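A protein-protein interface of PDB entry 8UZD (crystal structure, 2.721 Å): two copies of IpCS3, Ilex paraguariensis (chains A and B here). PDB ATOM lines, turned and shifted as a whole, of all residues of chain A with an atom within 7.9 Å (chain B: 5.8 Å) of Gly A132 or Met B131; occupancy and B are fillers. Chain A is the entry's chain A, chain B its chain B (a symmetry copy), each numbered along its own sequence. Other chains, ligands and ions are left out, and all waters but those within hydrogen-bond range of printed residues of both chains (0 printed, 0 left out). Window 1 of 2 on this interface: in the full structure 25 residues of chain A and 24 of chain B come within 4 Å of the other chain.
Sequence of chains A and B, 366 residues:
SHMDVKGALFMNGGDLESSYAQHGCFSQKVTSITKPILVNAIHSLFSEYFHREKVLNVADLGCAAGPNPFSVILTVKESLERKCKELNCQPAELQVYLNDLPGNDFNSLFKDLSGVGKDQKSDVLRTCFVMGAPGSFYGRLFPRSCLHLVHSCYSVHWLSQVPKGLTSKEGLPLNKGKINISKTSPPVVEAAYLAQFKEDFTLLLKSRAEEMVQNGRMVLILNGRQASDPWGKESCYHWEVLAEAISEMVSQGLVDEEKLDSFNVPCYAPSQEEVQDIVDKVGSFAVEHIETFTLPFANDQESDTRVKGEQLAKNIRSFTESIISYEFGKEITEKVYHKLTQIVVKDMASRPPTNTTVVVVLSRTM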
ATOM      1  N   CYS A  63      -5.856  23.732 -21.516  1.00  0.00           N
ATOM      2  CA  CYS A  63      -5.988  24.616 -22.662  1.00  0.00           C
ATOM      3  C   CYS A  63      -4.818  25.597 -22.728  1.00  0.00           C
ATOM      4  O   CYS A  63      -4.578  26.190 -23.778  1.00  0.00           O
ATOM      5  CB  CYS A  63      -7.293  25.403 -22.584  1.00  0.00           C
ATOM      6  SG  CYS A  63      -7.468  26.357 -21.050  1.00  0.00           S
ATOM      7  N   GLN A  95     -21.660  25.593 -25.682  1.00  0.00           N
ATOM      8  CA  GLN A  95     -20.955  25.921 -24.453  1.00  0.00           C
ATOM      9  C   GLN A  95     -19.594  25.233 -24.471  1.00  0.00           C
ATOM     10  O   GLN A  95     -19.522  24.008 -24.613  1.00  0.00           O
ATOM     11  CB  GLN A  95     -21.780  25.551 -23.216  1.00  0.00           C
ATOM     12  CG  GLN A  95     -21.035  25.786 -21.908  1.00  0.00           C
ATOM     13  CD  GLN A  95     -21.865  25.630 -20.659  1.00  0.00           C
ATOM     14  OE1 GLN A  95     -21.789  26.452 -19.743  1.00  0.00           O
ATOM     15  NE2 GLN A  95     -22.649  24.563 -20.603  1.00  0.00           N
ATOM     16  N   VAL A  96     -18.532  26.037 -24.315  1.00  0.00           N
ATOM     17  CA  VAL A  96     -17.171  25.517 -24.313  1.00  0.00           C
ATOM     18  C   VAL A  96     -16.531  25.798 -22.958  1.00  0.00           C
ATOM     19  O   VAL A  96     -16.386  26.958 -22.563  1.00  0.00           O
ATOM     20  CB  VAL A  96     -16.326  26.095 -25.471  1.00  0.00           C
ATOM     21  CG1 VAL A  96     -14.871  25.638 -25.419  1.00  0.00           C
ATOM     22  CG2 VAL A  96     -16.940  25.758 -26.824  1.00  0.00           C
ATOM     23  N   TYR A  97     -16.150  24.713 -22.274  1.00  0.00           N
ATOM     24  CA  TYR A  97     -15.355  24.782 -21.058  1.00  0.00           C
ATOM     25  C   TYR A  97     -13.877  24.700 -21.425  1.00  0.00           C
ATOM     26  O   TYR A  97     -13.457  23.726 -22.057  1.00  0.00           O
ATOM     27  CB  TYR A  97     -15.650  23.574 -20.171  1.00  0.00           C
ATOM     28  CG  TYR A  97     -17.037  23.546 -19.595  1.00  0.00           C
ATOM     29  CD1 TYR A  97     -17.362  24.288 -18.465  1.00  0.00           C
ATOM     30  CD2 TYR A  97     -18.030  22.769 -20.171  1.00  0.00           C
ATOM     31  CE1 TYR A  97     -18.639  24.254 -17.922  1.00  0.00           C
ATOM     32  CE2 TYR A  97     -19.315  22.742 -19.650  1.00  0.00           C
ATOM     33  CZ  TYR A  97     -19.612  23.472 -18.516  1.00  0.00           C
ATOM     34  OH  TYR A  97     -20.871  23.426 -18.007  1.00  0.00           O
ATOM     35  N   LEU A  98     -13.102  25.702 -20.989  1.00  0.00           N
ATOM     36  CA  LEU A  98     -11.656  25.671 -21.146  1.00  0.00           C
ATOM     37  C   LEU A  98     -10.976  25.319 -19.824  1.00  0.00           C
ATOM     38  O   LEU A  98     -10.747  26.206 -19.003  1.00  0.00           O
ATOM     39  CB  LEU A  98     -11.189  27.046 -21.622  1.00  0.00           C
ATOM     40  CG  LEU A  98     -11.715  27.501 -22.979  1.00  0.00           C
ATOM     41  CD1 LEU A  98     -10.999  28.777 -23.408  1.00  0.00           C
ATOM     42  CD2 LEU A  98     -11.581  26.396 -24.013  1.00  0.00           C
ATOM     43  N   ASN A  99     -10.605  24.039 -19.653  1.00  0.00           N
ATOM     44  CA  ASN A  99      -9.980  23.561 -18.425  1.00  0.00           C
ATOM     45  C   ASN A  99      -8.465  23.753 -18.456  1.00  0.00           C
ATOM     46  O   ASN A  99      -7.830  23.514 -19.482  1.00  0.00           O
ATOM     47  CB  ASN A  99     -10.307  22.093 -18.143  1.00  0.00           C
ATOM     48  CG  ASN A  99      -9.324  21.455 -17.181  1.00  0.00           C
ATOM     49  OD1 ASN A  99      -8.429  20.733 -17.602  1.00  0.00           O
ATOM     50  ND2 ASN A  99      -9.445  21.747 -15.895  1.00  0.00           N
ATOM     51  N   ASP A 100      -7.913  24.185 -17.311  1.00  0.00           N
ATOM     52  CA  ASP A 100      -6.490  24.148 -16.987  1.00  0.00           C
ATOM     53  C   ASP A 100      -6.318  24.312 -15.468  1.00  0.00           C
ATOM     54  O   ASP A 100      -7.278  24.635 -14.767  1.00  0.00           O
ATOM     55  CB  ASP A 100      -5.675  25.138 -17.827  1.00  0.00           C
ATOM     56  CG  ASP A 100      -4.209  24.737 -17.977  1.00  0.00           C
ATOM     57  OD1 ASP A 100      -3.515  24.666 -16.942  1.00  0.00           O
ATOM     58  OD2 ASP A 100      -3.766  24.479 -19.128  1.00  0.00           O
ATOM     59  N   PHE A 106      -5.577  32.621 -17.049  1.00  0.00           N
ATOM     60  CA  PHE A 106      -6.920  32.800 -17.569  1.00  0.00           C
ATOM     61  C   PHE A 106      -7.170  34.272 -17.898  1.00  0.00           C
ATOM     62  O   PHE A 106      -7.943  34.581 -18.803  1.00  0.00           O
ATOM     63  CB  PHE A 106      -7.959  32.227 -16.608  1.00  0.00           C
ATOM     64  CG  PHE A 106      -7.996  30.720 -16.503  1.00  0.00           C
ATOM     65  CD1 PHE A 106      -8.754  29.962 -17.388  1.00  0.00           C
ATOM     66  CD2 PHE A 106      -7.300  30.055 -15.499  1.00  0.00           C
ATOM     67  CE1 PHE A 106      -8.813  28.579 -17.282  1.00  0.00           C
ATOM     68  CE2 PHE A 106      -7.349  28.668 -15.403  1.00  0.00           C
ATOM     69  CZ  PHE A 106      -8.111  27.931 -16.291  1.00  0.00           C
ATOM     70  N   LEU A 109      -6.007  34.753 -21.470  1.00  0.00           N
ATOM     71  CA  LEU A 109      -6.875  33.939 -22.307  1.00  0.00           C
ATOM     72  C   LEU A 109      -8.199  34.662 -22.549  1.00  0.00           C
ATOM     73  O   LEU A 109      -8.620  34.806 -23.694  1.00  0.00           O
ATOM     74  CB  LEU A 109      -7.098  32.579 -21.631  1.00  0.00           C
ATOM     75  CG  LEU A 109      -7.934  31.569 -22.417  1.00  0.00           C
ATOM     76  CD1 LEU A 109      -7.239  31.155 -23.700  1.00  0.00           C
ATOM     77  CD2 LEU A 109      -8.215  30.343 -21.574  1.00  0.00           C
ATOM     78  N   PHE A 110      -8.819  35.149 -21.466  1.00  0.00           N
ATOM     79  CA  PHE A 110     -10.135  35.767 -21.516  1.00  0.00           C
ATOM     80  C   PHE A 110     -10.094  37.099 -22.258  1.00  0.00           C
ATOM     81  O   PHE A 110     -11.080  37.469 -22.899  1.00  0.00           O
ATOM     82  CB  PHE A 110     -10.704  35.965 -20.109  1.00  0.00           C
ATOM     83  CG  PHE A 110     -11.135  34.696 -19.418  1.00  0.00           C
ATOM     84  CD1 PHE A 110     -11.289  33.515 -20.132  1.00  0.00           C
ATOM     85  CD2 PHE A 110     -11.416  34.689 -18.054  1.00  0.00           C
ATOM     86  CE1 PHE A 110     -11.677  32.352 -19.490  1.00  0.00           C
ATOM     87  CE2 PHE A 110     -11.813  33.523 -17.414  1.00  0.00           C
ATOM     88  CZ  PHE A 110     -11.941  32.359 -18.135  1.00  0.00           C
ATOM     89  N   LEU A 113      -9.891  36.322 -25.975  1.00  0.00           N
ATOM     90  CA  LEU A 113     -11.129  35.754 -26.492  1.00  0.00           C
ATOM     91  C   LEU A 113     -12.146  36.864 -26.756  1.00  0.00           C
ATOM     92  O   LEU A 113     -13.197  36.614 -27.346  1.00  0.00           O
ATOM     93  CB  LEU A 113     -11.693  34.714 -25.510  1.00  0.00           C
ATOM     94  CG  LEU A 113     -11.075  33.314 -25.564  1.00  0.00           C
ATOM     95  CD1 LEU A 113     -11.384  32.564 -24.283  1.00  0.00           C
ATOM     96  CD2 LEU A 113     -11.587  32.525 -26.754  1.00  0.00           C
ATOM     97  N   PHE A 129     -20.862  30.356 -25.582  1.00  0.00           N
ATOM     98  CA  PHE A 129     -20.630  30.648 -24.179  1.00  0.00           C
ATOM     99  C   PHE A 129     -19.370  29.931 -23.711  1.00  0.00           C
ATOM    100  O   PHE A 129     -19.378  28.708 -23.557  1.00  0.00           O
ATOM    101  CB  PHE A 129     -21.857  30.239 -23.363  1.00  0.00           C
ATOM    102  CG  PHE A 129     -23.159  30.764 -23.910  1.00  0.00           C
ATOM    103  CD1 PHE A 129     -23.342  32.129 -24.118  1.00  0.00           C
ATOM    104  CD2 PHE A 129     -24.196  29.900 -24.230  1.00  0.00           C
ATOM    105  CE1 PHE A 129     -24.538  32.621 -24.632  1.00  0.00           C
ATOM    106  CE2 PHE A 129     -25.390  30.391 -24.740  1.00  0.00           C
ATOM    107  CZ  PHE A 129     -25.566  31.748 -24.926  1.00  0.00           C
ATOM    108  N   VAL A 130     -18.309  30.719 -23.482  1.00  0.00           N
ATOM    109  CA  VAL A 130     -16.978  30.211 -23.200  1.00  0.00           C
ATOM    110  C   VAL A 130     -16.653  30.432 -21.726  1.00  0.00           C
ATOM    111  O   VAL A 130     -16.693  31.561 -21.252  1.00  0.00           O
ATOM    112  CB  VAL A 130     -15.927  30.869 -24.119  1.00  0.00           C
ATOM    113  CG1 VAL A 130     -14.508  30.431 -23.784  1.00  0.00           C
ATOM    114  CG2 VAL A 130     -16.231  30.587 -25.582  1.00  0.00           C
ATOM    115  N   MET A 131     -16.300  29.341 -21.031  1.00  0.00           N
ATOM    116  CA  MET A 131     -16.048  29.340 -19.596  1.00  0.00           C
ATOM    117  C   MET A 131     -14.605  28.929 -19.306  1.00  0.00           C
ATOM    118  O   MET A 131     -13.988  28.191 -20.078  1.00  0.00           O
ATOM    119  CB  MET A 131     -16.964  28.342 -18.877  1.00  0.00           C
ATOM    120  CG  MET A 131     -18.421  28.440 -19.259  1.00  0.00           C
ATOM    121  SD  MET A 131     -19.147  30.021 -18.810  1.00  0.00           S
ATOM    122  CE  MET A 131     -20.694  29.924 -19.707  1.00  0.00           C
ATOM    123  N   GLY A 132     -14.100  29.394 -18.155  1.00  0.00           N
ATOM    124  CA  GLY A 132     -12.879  28.871 -17.565  1.00  0.00           C
ATOM    125  C   GLY A 132     -13.213  27.847 -16.482  1.00  0.00           C
ATOM    126  O   GLY A 132     -14.064  28.101 -15.623  1.00  0.00           O
ATOM    127  N   ALA A 133     -12.553  26.684 -16.549  1.00  0.00           N
ATOM    128  CA  ALA A 133     -12.795  25.599 -15.614  1.00  0.00           C
ATOM    129  C   ALA A 133     -11.484  25.219 -14.936  1.00  0.00           C
ATOM    130  O   ALA A 133     -10.819  24.271 -15.353  1.00  0.00           O
ATOM    131  CB  ALA A 133     -13.413  24.431 -16.336  1.00  0.00           C
ATOM    132  N   PRO A 134     -11.064  25.966 -13.885  1.00  0.00           N
ATOM    133  CA  PRO A 134      -9.821  25.670 -13.167  1.00  0.00           C
ATOM    134  C   PRO A 134      -9.944  24.397 -12.336  1.00  0.00           C
ATOM    135  O   PRO A 134     -10.998  24.125 -11.784  1.00  0.00           O
ATOM    136  CB  PRO A 134      -9.627  26.901 -12.267  1.00  0.00           C
ATOM    137  CG  PRO A 134     -11.023  27.446 -12.056  1.00  0.00           C
ATOM    138  CD  PRO A 134     -11.761  27.146 -13.345  1.00  0.00           C
ATOM    139  N   GLY A 135      -8.853  23.622 -12.262  1.00  0.00           N
ATOM    140  CA  GLY A 135      -8.815  22.332 -11.592  1.00  0.00           C
ATOM    141  C   GLY A 135      -7.945  21.349 -12.372  1.00  0.00           C
ATOM    142  O   GLY A 135      -7.487  21.661 -13.469  1.00  0.00           O
ATOM    143  N   LEU A 141     -14.726  17.345 -12.964  1.00  0.00           N
ATOM    144  CA  LEU A 141     -14.599  18.758 -13.294  1.00  0.00           C
ATOM    145  C   LEU A 141     -15.945  19.361 -13.705  1.00  0.00           C
ATOM    146  O   LEU A 141     -16.101  20.586 -13.680  1.00  0.00           O
ATOM    147  CB  LEU A 141     -13.587  18.926 -14.425  1.00  0.00           C
ATOM    148  CG  LEU A 141     -12.116  18.953 -14.020  1.00  0.00           C
ATOM    149  CD1 LEU A 141     -11.234  18.838 -15.266  1.00  0.00           C
ATOM    150  CD2 LEU A 141     -11.773  20.204 -13.229  1.00  0.00           C
ATOM    151  N   PHE A 142     -16.899  18.494 -14.079  1.00  0.00           N
ATOM    152  CA  PHE A 142     -18.131  18.894 -14.748  1.00  0.00           C
ATOM    153  C   PHE A 142     -19.290  18.007 -14.301  1.00  0.00           C
ATOM    154  O   PHE A 142     -19.078  16.876 -13.871  1.00  0.00           O
ATOM    155  CB  PHE A 142     -17.992  18.730 -16.269  1.00  0.00           C
ATOM    156  CG  PHE A 142     -16.784  19.407 -16.862  1.00  0.00           C
ATOM    157  CD1 PHE A 142     -16.727  20.788 -16.964  1.00  0.00           C
ATOM    158  CD2 PHE A 142     -15.692  18.665 -17.278  1.00  0.00           C
ATOM    159  CE1 PHE A 142     -15.605  21.415 -17.480  1.00  0.00           C
ATOM    160  CE2 PHE A 142     -14.580  19.293 -17.818  1.00  0.00           C
ATOM    161  CZ  PHE A 142     -14.537  20.664 -17.920  1.00  0.00           C
ATOM    162  N   PRO A 143     -20.552  18.483 -14.419  1.00  0.00           N
ATOM    163  CA  PRO A 143     -21.721  17.669 -14.080  1.00  0.00           C
ATOM    164  C   PRO A 143     -21.720  16.337 -14.817  1.00  0.00           C
ATOM    165  O   PRO A 143     -21.094  16.215 -15.869  1.00  0.00           O
ATOM    166  CB  PRO A 143     -22.880  18.502 -14.631  1.00  0.00           C
ATOM    167  CG  PRO A 143     -22.381  19.926 -14.528  1.00  0.00           C
ATOM    168  CD  PRO A 143     -20.909  19.845 -14.857  1.00  0.00           C
ATOM    169  N   GLN B  95     -22.977  23.356  -9.696  1.00  0.00           N
ATOM    170  CA  GLN B  95     -22.173  24.107 -10.643  1.00  0.00           C
ATOM    171  C   GLN B  95     -22.393  25.589 -10.391  1.00  0.00           C
ATOM    172  O   GLN B  95     -23.527  26.054 -10.421  1.00  0.00           O
ATOM    173  CB  GLN B  95     -22.489  23.712 -12.087  1.00  0.00           C
ATOM    174  CG  GLN B  95     -21.751  24.558 -13.116  1.00  0.00           C
ATOM    175  CD  GLN B  95     -21.837  24.043 -14.535  1.00  0.00           C
ATOM    176  OE1 GLN B  95     -20.833  23.943 -15.234  1.00  0.00           O
ATOM    177  NE2 GLN B  95     -23.038  23.722 -14.987  1.00  0.00           N
ATOM    178  N   VAL B  96     -21.296  26.312 -10.136  1.00  0.00           N
ATOM    179  CA  VAL B  96     -21.355  27.743  -9.878  1.00  0.00           C
ATOM    180  C   VAL B  96     -20.559  28.475 -10.955  1.00  0.00           C
ATOM    181  O   VAL B  96     -19.354  28.274 -11.081  1.00  0.00           O
ATOM    182  CB  VAL B  96     -20.857  28.115  -8.466  1.00  0.00           C
ATOM    183  CG1 VAL B  96     -20.946  29.618  -8.223  1.00  0.00           C
ATOM    184  CG2 VAL B  96     -21.602  27.357  -7.381  1.00  0.00           C
ATOM    185  N   TYR B  97     -21.264  29.317 -11.719  1.00  0.00           N
ATOM    186  CA  TYR B  97     -20.675  30.227 -12.683  1.00  0.00           C
ATOM    187  C   TYR B  97     -20.381  31.552 -11.996  1.00  0.00           C
ATOM    188  O   TYR B  97     -21.292  32.172 -11.464  1.00  0.00           O
ATOM    189  CB  TYR B  97     -21.677  30.538 -13.794  1.00  0.00           C
ATOM    190  CG  TYR B  97     -21.977  29.376 -14.702  1.00  0.00           C
ATOM    191  CD1 TYR B  97     -21.116  29.041 -15.741  1.00  0.00           C
ATOM    192  CD2 TYR B  97     -23.124  28.617 -14.541  1.00  0.00           C
ATOM    193  CE1 TYR B  97     -21.377  27.977 -16.590  1.00  0.00           C
ATOM    194  CE2 TYR B  97     -23.418  27.567 -15.397  1.00  0.00           C
ATOM    195  CZ  TYR B  97     -22.534  27.240 -16.416  1.00  0.00           C
ATOM    196  OH  TYR B  97     -22.787  26.197 -17.256  1.00  0.00           O
ATOM    197  N   LEU B  98     -19.111  31.980 -12.035  1.00  0.00           N
ATOM    198  CA  LEU B  98     -18.721  33.284 -11.527  1.00  0.00           C
ATOM    199  C   LEU B  98     -18.510  34.264 -12.688  1.00  0.00           C
ATOM    200  O   LEU B  98     -17.444  34.296 -13.302  1.00  0.00           O
ATOM    201  CB  LEU B  98     -17.439  33.110 -10.708  1.00  0.00           C
ATOM    202  CG  LEU B  98     -17.536  32.217  -9.472  1.00  0.00           C
ATOM    203  CD1 LEU B  98     -16.307  32.381  -8.600  1.00  0.00           C
ATOM    204  CD2 LEU B  98     -18.774  32.537  -8.653  1.00  0.00           C
ATOM    205  N   ASN B  99     -19.529  35.090 -12.966  1.00  0.00           N
ATOM    206  CA  ASN B  99     -19.490  36.044 -14.063  1.00  0.00           C
ATOM    207  C   ASN B  99     -18.857  37.362 -13.619  1.00  0.00           C
ATOM    208  O   ASN B  99     -19.137  37.859 -12.531  1.00  0.00           O
ATOM    209  CB  ASN B  99     -20.884  36.310 -14.642  1.00  0.00           C
ATOM    210  CG  ASN B  99     -20.948  37.611 -15.420  1.00  0.00           C
ATOM    211  OD1 ASN B  99     -21.445  38.612 -14.913  1.00  0.00           O
ATOM    212  ND2 ASN B  99     -20.400  37.626 -16.629  1.00  0.00           N
ATOM    213  N   PHE B 110      -9.267  32.479  -8.866  1.00  0.00           N
ATOM    214  CA  PHE B 110      -9.109  31.043  -9.026  1.00  0.00           C
ATOM    215  C   PHE B 110      -8.028  30.501  -8.097  1.00  0.00           C
ATOM    216  O   PHE B 110      -8.117  29.354  -7.664  1.00  0.00           O
ATOM    217  CB  PHE B 110      -8.780  30.695 -10.477  1.00  0.00           C
ATOM    218  CG  PHE B 110      -9.918  30.862 -11.452  1.00  0.00           C
ATOM    219  CD1 PHE B 110     -11.223  31.041 -11.016  1.00  0.00           C
ATOM    220  CD2 PHE B 110      -9.686  30.804 -12.820  1.00  0.00           C
ATOM    221  CE1 PHE B 110     -12.264  31.189 -11.923  1.00  0.00           C
ATOM    222  CE2 PHE B 110     -10.731  30.944 -13.724  1.00  0.00           C
ATOM    223  CZ  PHE B 110     -12.018  31.140 -13.276  1.00  0.00           C
ATOM    224  N   PHE B 129     -18.355  22.385  -8.762  1.00  0.00           N
ATOM    225  CA  PHE B 129     -17.664  22.749  -9.992  1.00  0.00           C
ATOM    226  C   PHE B 129     -17.836  24.247 -10.249  1.00  0.00           C
ATOM    227  O   PHE B 129     -18.924  24.709 -10.590  1.00  0.00           O
ATOM    228  CB  PHE B 129     -18.161  21.884 -11.161  1.00  0.00           C
ATOM    229  CG  PHE B 129     -18.261  20.410 -10.836  1.00  0.00           C
ATOM    230  CD1 PHE B 129     -17.156  19.701 -10.370  1.00  0.00           C
ATOM    231  CD2 PHE B 129     -19.465  19.731 -10.971  1.00  0.00           C
ATOM    232  CE1 PHE B 129     -17.243  18.352 -10.050  1.00  0.00           C
ATOM    233  CE2 PHE B 129     -19.560  18.380 -10.648  1.00  0.00           C
ATOM    234  CZ  PHE B 129     -18.445  17.691 -10.192  1.00  0.00           C
ATOM    235  N   VAL B 130     -16.731  24.986 -10.090  1.00  0.00           N
ATOM    236  CA  VAL B 130     -16.705  26.438 -10.117  1.00  0.00           C
ATOM    237  C   VAL B 130     -16.060  26.897 -11.420  1.00  0.00           C
ATOM    238  O   VAL B 130     -14.927  26.521 -11.713  1.00  0.00           O
ATOM    239  CB  VAL B 130     -15.939  26.989  -8.898  1.00  0.00           C
ATOM    240  CG1 VAL B 130     -15.814  28.508  -8.928  1.00  0.00           C
ATOM    241  CG2 VAL B 130     -16.563  26.525  -7.592  1.00  0.00           C
ATOM    242  N   MET B 131     -16.785  27.744 -12.165  1.00  0.00           N
ATOM    243  CA  MET B 131     -16.384  28.202 -13.485  1.00  0.00           C
ATOM    244  C   MET B 131     -16.236  29.722 -13.490  1.00  0.00           C
ATOM    245  O   MET B 131     -16.895  30.425 -12.729  1.00  0.00           O
ATOM    246  CB  MET B 131     -17.437  27.837 -14.536  1.00  0.00           C
ATOM    247  CG  MET B 131     -17.889  26.406 -14.513  1.00  0.00           C
ATOM    248  SD  MET B 131     -16.552  25.258 -14.935  1.00  0.00           S
ATOM    249  CE  MET B 131     -17.312  23.692 -14.500  1.00  0.00           C
ATOM    250  N   GLY B 132     -15.380  30.220 -14.391  1.00  0.00           N
ATOM    251  CA  GLY B 132     -15.346  31.625 -14.756  1.00  0.00           C
ATOM    252  C   GLY B 132     -16.142  31.861 -16.037  1.00  0.00           C
ATOM    253  O   GLY B 132     -15.972  31.142 -17.018  1.00  0.00           O
ATOM    254  N   ALA B 133     -17.023  32.869 -16.003  1.00  0.00           N
ATOM    255  CA  ALA B 133     -17.848  33.232 -17.140  1.00  0.00           C
ATOM    256  C   ALA B 133     -17.605  34.700 -17.481  1.00  0.00           C
ATOM    257  O   ALA B 133     -18.378  35.575 -17.075  1.00  0.00           O
ATOM    258  CB  ALA B 133     -19.292  32.971 -16.816  1.00  0.00           C
ATOM    259  N   PRO B 134     -16.529  35.007 -18.250  1.00  0.00           N
ATOM    260  CA  PRO B 134     -16.253  36.379 -18.692  1.00  0.00           C
ATOM    261  C   PRO B 134     -17.281  36.881 -19.706  1.00  0.00           C
ATOM    262  O   PRO B 134     -17.773  36.105 -20.523  1.00  0.00           O
ATOM    263  CB  PRO B 134     -14.859  36.275 -19.338  1.00  0.00           C
ATOM    264  CG  PRO B 134     -14.768  34.831 -19.798  1.00  0.00           C
ATOM    265  CD  PRO B 134     -15.550  34.038 -18.767  1.00  0.00           C
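The side-chain hydroxyl (OH) of Tyr A97 lies within hydrogen-bond range of the side-chain amide oxygen (OE1) of Gln B95 (2.8 Å). The side-chain amide oxygen of Gln A95 is in hydrogen-bond range of the side-chain hydroxyl of Tyr B97. The side-chain hydroxyl of Tyr A97 is in hydrogen-bond range of the side-chain hydroxyl of Tyr B97 (3.5 Å). The backbone carbonyl oxygen (O) of Gly A132 sits at hydrogen-bond distance from the backbone NH (N) of Gly B132 (2.8 Å).
Printed residues of chain B within 4 Å of Phe A110: Pro B134 (3.7 Å). Printed residues of chain A within 4 Å of Ala B133: Met A131 (3.6 Å). The nearest residue of chain A that does not touch Met B131 is Met A131 (4.4 Å). The nearest printed residue of chain B that does not touch Pro A143 is Met B131 (5.3 Å).
Of the 12 printed residues of chain B, 9 touch a printed residue of chain A. Hydrophobic or aromatic side chains of chain B that line the printed part of chain A: Tyr B97, Phe B110, Phe B129, Met B131, Ala B133 and Pro B134. Among the printed residues, 21 pairs touch across the chains. Among the printed residues, no Asp or Glu carboxylate lies within 4 Å of a Lys or Arg side-chain nitrogen of the other chain.
Tyr A97 touches its own counterpart, Tyr B97. Phe A110 touches Pro B134, and with the chains exchanged Pro A134 touches Phe B110. Val A130 touches Pro B134, and with the chains exchanged Pro A134 touches Val B130. Met A131 touches Ala B133, and with the chains exchanged Ala A133 touches Met B131. 12 positions are printed for both chains. Of the 21 pairs that touch across the chains among the printed residues, 14 have their exchanged pair printed and touching as well.
Among the printed residues, pairs that only touch across the chains: Tyr A97 with Met B131, Phe A106 with Phe B110, Phe A110 with Pro B134, Val A130 with Pro B134, Met A131 with Tyr B97, Met A131 with Gly B132, Met A131 with Ala B133, Gly A132 with Met B131, Ala A133 with Met B131, Pro A134 with Phe B110, Pro A134 with Val B130, Leu A141 with Phe B129, Leu A141 with Met B131, Phe A142 with Phe B129, Phe A142 with Met B131, Pro A143 with Gln B95 and Pro A143 with Phe B129.
O of Ala B133 lies within hydrogen-bond range of ND2 of Asn B99 (2.9 Å). The backbone carbonyl oxygen (O) of Ala A133 is in hydrogen-bond range of the side-chain amide nitrogen (ND2) of Asn A99 (2.9 Å). The backbone NH (N) of Met B131 is in hydrogen-bond range of the backbone carbonyl oxygen (O) of Val B96 (2.8 Å). The side-chain amide nitrogen (NE2) of Gln B95 lies within hydrogen-bond range of the side-chain hydroxyl (OH) of Tyr B97 (3.4 Å). The backbone NH (N) of Met A131 is in hydrogen-bond range of the backbone carbonyl oxygen (O) of Val A96 (2.8 Å). The backbone carbonyl oxygen (O) of Met A131 sits at hydrogen-bond distance from the backbone NH (N) of Leu A98.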
